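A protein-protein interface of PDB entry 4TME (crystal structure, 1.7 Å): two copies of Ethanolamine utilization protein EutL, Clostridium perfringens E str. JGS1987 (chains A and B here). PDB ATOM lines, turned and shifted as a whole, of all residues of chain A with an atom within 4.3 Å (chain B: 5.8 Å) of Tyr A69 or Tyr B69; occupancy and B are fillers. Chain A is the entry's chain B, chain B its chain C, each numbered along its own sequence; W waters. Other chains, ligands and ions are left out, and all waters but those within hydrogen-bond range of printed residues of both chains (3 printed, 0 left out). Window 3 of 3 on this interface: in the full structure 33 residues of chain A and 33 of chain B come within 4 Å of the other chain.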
ATOM      1  N   SER A  67      -7.355  -1.545  17.581  1.00  0.00           N
ATOM      2  CA  SER A  67      -8.713  -1.413  17.091  1.00  0.00           C
ATOM      3  C   SER A  67      -9.699  -0.964  18.176  1.00  0.00           C
ATOM      4  O   SER A  67      -9.490  -1.251  19.350  1.00  0.00           O
ATOM      5  CB  SER A  67      -9.196  -2.756  16.524  1.00  0.00           C
ATOM      6  OG  SER A  67      -8.337  -3.205  15.465  1.00  0.00           O
ATOM      7  N   MET A  68     -10.795  -0.333  17.754  1.00  0.00           N
ATOM      8  CA  MET A  68     -11.799   0.214  18.672  1.00  0.00           C
ATOM      9  C   MET A  68     -12.950  -0.763  18.915  1.00  0.00           C
ATOM     10  O   MET A  68     -13.399  -1.466  17.999  1.00  0.00           O
ATOM     11  CB  MET A  68     -12.383   1.534  18.154  1.00  0.00           C
ATOM     12  CG  MET A  68     -11.365   2.589  17.794  1.00  0.00           C
ATOM     13  SD  MET A  68     -10.572   3.218  19.296  1.00  0.00           S
ATOM     14  CE  MET A  68      -8.894   2.847  18.979  1.00  0.00           C
ATOM     15  N   TYR A  69     -13.433  -0.794  20.150  1.00  0.00           N
ATOM     16  CA  TYR A  69     -14.504  -1.728  20.516  1.00  0.00           C
ATOM     17  C   TYR A  69     -15.773  -1.457  19.718  1.00  0.00           C
ATOM     18  O   TYR A  69     -16.267  -0.335  19.668  1.00  0.00           O
ATOM     19  CB  TYR A  69     -14.824  -1.656  22.009  1.00  0.00           C
ATOM     20  CG  TYR A  69     -13.703  -2.168  22.858  1.00  0.00           C
ATOM     21  CD1 TYR A  69     -13.424  -3.530  22.953  1.00  0.00           C
ATOM     22  CD2 TYR A  69     -12.871  -1.280  23.545  1.00  0.00           C
ATOM     23  CE1 TYR A  69     -12.370  -3.996  23.714  1.00  0.00           C
ATOM     24  CE2 TYR A  69     -11.808  -1.740  24.279  1.00  0.00           C
ATOM     25  CZ  TYR A  69     -11.567  -3.095  24.369  1.00  0.00           C
ATOM     26  OH  TYR A  69     -10.513  -3.546  25.122  1.00  0.00           O
ATOM     27  N   ALA A  70     -16.270  -2.523  19.085  1.00  0.00           N
ATOM     28  CA  ALA A  70     -17.520  -2.550  18.312  1.00  0.00           C
ATOM     29  C   ALA A  70     -17.497  -1.832  16.953  1.00  0.00           C
ATOM     30  O   ALA A  70     -18.530  -1.696  16.328  1.00  0.00           O
ATOM     31  CB  ALA A  70     -18.683  -2.030  19.170  1.00  0.00           C
ATOM     32  N   GLY A  71     -16.318  -1.412  16.494  1.00  0.00           N
ATOM     33  CA  GLY A  71     -16.121  -0.990  15.125  1.00  0.00           C
ATOM     34  C   GLY A  71     -16.602   0.415  14.795  1.00  0.00           C
ATOM     35  O   GLY A  71     -17.225   1.120  15.609  1.00  0.00           O
ATOM     36  N   PRO A 179     -14.116 -12.710  19.760  1.00  0.00           N
ATOM     37  CA  PRO A 179     -14.055 -11.442  19.046  1.00  0.00           C
ATOM     38  C   PRO A 179     -12.722 -10.740  19.224  1.00  0.00           C
ATOM     39  O   PRO A 179     -12.160 -10.745  20.340  1.00  0.00           O
ATOM     40  CB  PRO A 179     -15.147 -10.608  19.723  1.00  0.00           C
ATOM     41  CG  PRO A 179     -15.087 -11.046  21.143  1.00  0.00           C
ATOM     42  CD  PRO A 179     -14.781 -12.559  21.069  1.00  0.00           C
ATOM     43  N   THR A 180     -12.249 -10.120  18.153  1.00  0.00           N
ATOM     44  CA  THR A 180     -11.314  -9.001  18.322  1.00  0.00           C
ATOM     45  C   THR A 180     -12.149  -7.767  18.729  1.00  0.00           C
ATOM     46  O   THR A 180     -13.386  -7.855  18.846  1.00  0.00           O
ATOM     47  CB  THR A 180     -10.525  -8.748  17.062  1.00  0.00           C
ATOM     48  OG1 THR A 180     -11.427  -8.464  16.007  1.00  0.00           O
ATOM     49  CG2 THR A 180      -9.680  -9.995  16.699  1.00  0.00           C
ATOM     50  N   GLU A 181     -11.518  -6.607  18.935  1.00  0.00           N
ATOM     51  CA  GLU A 181     -12.278  -5.452  19.425  1.00  0.00           C
ATOM     52  C   GLU A 181     -13.488  -5.094  18.540  1.00  0.00           C
ATOM     53  O   GLU A 181     -14.552  -4.728  19.080  1.00  0.00           O
ATOM     54  CB  GLU A 181     -11.360  -4.221  19.562  1.00  0.00           C
ATOM     55  CG  GLU A 181     -10.371  -4.336  20.685  1.00  0.00           C
ATOM     56  CD  GLU A 181      -9.068  -5.044  20.302  1.00  0.00           C
ATOM     57  OE1 GLU A 181      -8.937  -5.535  19.163  1.00  0.00           O
ATOM     58  OE2 GLU A 181      -8.171  -5.103  21.178  1.00  0.00           O
ATOM     59  N   ASN A 183     -15.241  -7.114  16.742  1.00  0.00           N
ATOM     60  CA  ASN A 183     -16.099  -8.303  16.631  1.00  0.00           C
ATOM     61  C   ASN A 183     -15.922  -8.993  15.291  1.00  0.00           C
ATOM     62  O   ASN A 183     -16.868  -9.547  14.715  1.00  0.00           O
ATOM     63  CB  ASN A 183     -17.569  -7.950  16.897  1.00  0.00           C
ATOM     64  CG  ASN A 183     -17.768  -7.426  18.309  1.00  0.00           C
ATOM     65  OD1 ASN A 183     -17.253  -7.990  19.266  1.00  0.00           O
ATOM     66  ND2 ASN A 183     -18.512  -6.345  18.444  1.00  0.00           N
ATOM     67  N   ARG B  66     -17.651 -17.482  23.356  1.00  0.00           N
ATOM     68  CA  ARG B  66     -17.338 -16.073  23.627  1.00  0.00           C
ATOM     69  C   ARG B  66     -18.445 -15.139  23.173  1.00  0.00           C
ATOM     70  O   ARG B  66     -19.099 -15.387  22.150  1.00  0.00           O
ATOM     71  CB  ARG B  66     -16.041 -15.647  22.928  1.00  0.00           C
ATOM     72  CG  ARG B  66     -14.739 -16.312  23.388  1.00  0.00           C
ATOM     73  CD  ARG B  66     -14.313 -15.865  24.777  1.00  0.00           C
ATOM     74  NE  ARG B  66     -14.272 -14.394  24.921  1.00  0.00           N
ATOM     75  CZ  ARG B  66     -13.325 -13.591  24.432  1.00  0.00           C
ATOM     76  NH1 ARG B  66     -12.293 -14.078  23.761  1.00  0.00           N
ATOM     77  NH2 ARG B  66     -13.398 -12.270  24.629  1.00  0.00           N
ATOM     78  N   SER B  67     -18.611 -14.053  23.931  1.00  0.00           N
ATOM     79  CA  SER B  67     -19.574 -13.001  23.648  1.00  0.00           C
ATOM     80  C   SER B  67     -18.952 -11.832  22.877  1.00  0.00           C
ATOM     81  O   SER B  67     -17.749 -11.580  22.997  1.00  0.00           O
ATOM     82  CB  SER B  67     -20.162 -12.478  24.972  1.00  0.00           C
ATOM     83  OG  SER B  67     -20.790 -13.556  25.670  1.00  0.00           O
ATOM     84  N   MET B  68     -19.786 -11.109  22.140  1.00  0.00           N
ATOM     85  CA  MET B  68     -19.336  -9.986  21.315  1.00  0.00           C
ATOM     86  C   MET B  68     -19.416  -8.645  22.052  1.00  0.00           C
ATOM     87  O   MET B  68     -20.382  -8.374  22.797  1.00  0.00           O
ATOM     88  CB  MET B  68     -20.163  -9.872  20.033  1.00  0.00           C
ATOM     89  CG  MET B  68     -20.182 -11.134  19.195  1.00  0.00           C
ATOM     90  SD  MET B  68     -18.567 -11.518  18.493  1.00  0.00           S
ATOM     91  CE  MET B  68     -18.253 -13.111  19.158  1.00  0.00           C
ATOM     92  N   TYR B  69     -18.448  -7.767  21.790  1.00  0.00           N
ATOM     93  CA  TYR B  69     -18.433  -6.460  22.476  1.00  0.00           C
ATOM     94  C   TYR B  69     -19.655  -5.623  22.129  1.00  0.00           C
ATOM     95  O   TYR B  69     -19.980  -5.421  20.957  1.00  0.00           O
ATOM     96  CB  TYR B  69     -17.139  -5.686  22.146  1.00  0.00           C
ATOM     97  CG  TYR B  69     -15.914  -6.362  22.669  1.00  0.00           C
ATOM     98  CD1 TYR B  69     -15.615  -6.340  24.039  1.00  0.00           C
ATOM     99  CD2 TYR B  69     -15.034  -7.018  21.816  1.00  0.00           C
ATOM    100  CE1 TYR B  69     -14.485  -6.951  24.526  1.00  0.00           C
ATOM    101  CE2 TYR B  69     -13.887  -7.643  22.306  1.00  0.00           C
ATOM    102  CZ  TYR B  69     -13.629  -7.609  23.669  1.00  0.00           C
ATOM    103  OH  TYR B  69     -12.512  -8.222  24.170  1.00  0.00           O
ATOM    104  N   ALA B  70     -20.364  -5.204  23.188  1.00  0.00           N
ATOM    105  CA  ALA B  70     -21.493  -4.276  23.162  1.00  0.00           C
ATOM    106  C   ALA B  70     -22.791  -4.907  22.673  1.00  0.00           C
ATOM    107  O   ALA B  70     -23.781  -4.212  22.517  1.00  0.00           O
ATOM    108  CB  ALA B  70     -21.162  -3.024  22.334  1.00  0.00           C
ATOM    109  N   GLY B  71     -22.792  -6.227  22.494  1.00  0.00           N
ATOM    110  CA  GLY B  71     -24.032  -6.973  22.299  1.00  0.00           C
ATOM    111  C   GLY B  71     -24.666  -6.936  20.913  1.00  0.00           C
ATOM    112  O   GLY B  71     -24.230  -6.216  20.001  1.00  0.00           O
ATOM    113  N   ASN B  74     -25.667  -3.921  18.672  1.00  0.00           N
ATOM    114  CA  ASN B  74     -24.540  -3.171  18.125  1.00  0.00           C
ATOM    115  C   ASN B  74     -23.704  -3.993  17.139  1.00  0.00           C
ATOM    116  O   ASN B  74     -22.647  -3.559  16.709  1.00  0.00           O
ATOM    117  CB  ASN B  74     -23.657  -2.647  19.261  1.00  0.00           C
ATOM    118  CG  ASN B  74     -24.332  -1.520  20.036  1.00  0.00           C
ATOM    119  OD1 ASN B  74     -24.815  -0.548  19.446  1.00  0.00           O
ATOM    120  ND2 ASN B  74     -24.418  -1.678  21.348  1.00  0.00           N
ATOM    121  N   GLU B 181     -18.492  -8.787  27.957  1.00  0.00           N
ATOM    122  CA  GLU B 181     -18.366  -8.137  26.651  1.00  0.00           C
ATOM    123  C   GLU B 181     -19.638  -7.403  26.249  1.00  0.00           C
ATOM    124  O   GLU B 181     -19.562  -6.325  25.650  1.00  0.00           O
ATOM    125  CB  GLU B 181     -17.989  -9.154  25.556  1.00  0.00           C
ATOM    126  CG  GLU B 181     -16.543  -9.651  25.652  1.00  0.00           C
ATOM    127  CD  GLU B 181     -16.330 -10.809  26.624  1.00  0.00           C
ATOM    128  OE1 GLU B 181     -17.287 -11.252  27.306  1.00  0.00           O
ATOM    129  OE2 GLU B 181     -15.178 -11.292  26.696  1.00  0.00           O
ATOM    130  N   THR B 182     -20.805  -7.945  26.619  1.00  0.00           N
ATOM    131  CA  THR B 182     -22.074  -7.349  26.230  1.00  0.00           C
ATOM    132  C   THR B 182     -22.578  -6.307  27.246  1.00  0.00           C
ATOM    133  O   THR B 182     -23.705  -5.842  27.116  1.00  0.00           O
ATOM    134  CB  THR B 182     -23.193  -8.403  26.046  1.00  0.00           C
ATOM    135  OG1 THR B 182     -23.484  -9.062  27.289  1.00  0.00           O
ATOM    136  CG2 THR B 182     -22.779  -9.458  24.991  1.00  0.00           C
HETATM  137  O   HOH W   1     -19.840  -4.713  16.420  1.00  0.00           O
HETATM  138  O   HOH W   2     -11.571 -10.720  23.011  1.00  0.00           O
HETATM  139  O   HOH W   3     -21.743  -6.153  18.914  1.00  0.00           O
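Tyr A69 touches its own counterpart, Tyr B69. Glu A181 touches Tyr B69, but with the chains exchanged Tyr A69 does not touch Glu B181 (7.3 Å).
NH2 of Arg B66 lies within salt-bridge range of OE2 of Glu B181 (2.9 Å). The backbone carbonyl oxygen (O) of Glu A181 sits at hydrogen-bond distance from the backbone NH (N) of Ala A70 (2.8 Å).
Of the 9 printed residues of chain A, 5 touch a printed residue of chain B. Hydrophobic or aromatic side chains of chain A within 4 Å of the printed part of chain B: Tyr A69 and Pro A179. Along chain A the printed residues that touch a printed residue of chain B span positions 69 to 183.
Water W3 lies within hydrogen-bond range of O of Gly B71 (2.7 Å), O of Tyr B69 (2.8 Å) and ND2 of Asn A183 (3.3 Å). Water W2 lies within hydrogen-bond range of the backbone carbonyl oxygen (O) of Pro A179 (2.7 Å), the guanidinium group (NH2) of Arg B66 (2.9 Å) and the side-chain hydroxyl (OH) of Tyr B69 (2.9 Å). Water W1 lies within hydrogen-bond range of the side-chain amide nitrogen (ND2) of Asn A183, the backbone carbonyl oxygen (O) of Asn B74 and the backbone carbonyl oxygen (O) of Ala A70.
Of chain A, only Tyr A69, Pro A179, Thr A180, Glu A181 and Asn A183 come within 4 Å of Tyr B69. Of the printed residues of chain B, Asn A183 touches Met B68 (3.5 Å) and Tyr B69 (2.8 Å). Of the printed residues of chain A, Arg B66 touches Pro A179 (3.8 Å). Of the printed residues of chain A, Met B68 touches Pro A179 and Asn A183. Printed residues of chain A within 4 Å of Ser B67: Pro A179. The nearest printed residue of chain B that does not touch Tyr A69 is Ala B70 (6.2 Å). The nearest printed residue of chain B that does not touch Pro A179 is Glu B181 (4.9 Å).
Tyr A69 touches Tyr B69. Arg B66 touches Pro A179. CG of Pro A179 touches O of Ser B67 (3.3 Å). Pro A179 touches Met B68. CG of Pro A179 touches CE2 of Tyr B69, 3.8 Å away. Tyr B69 touches Thr A180. Glu A181 touches Tyr B69. Met B68 touches Asn A183 (CA to OD1, 3.5 Å).
N of Tyr B69 lies within hydrogen-bond range of OD1 of Asn A183 (2.8 Å).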
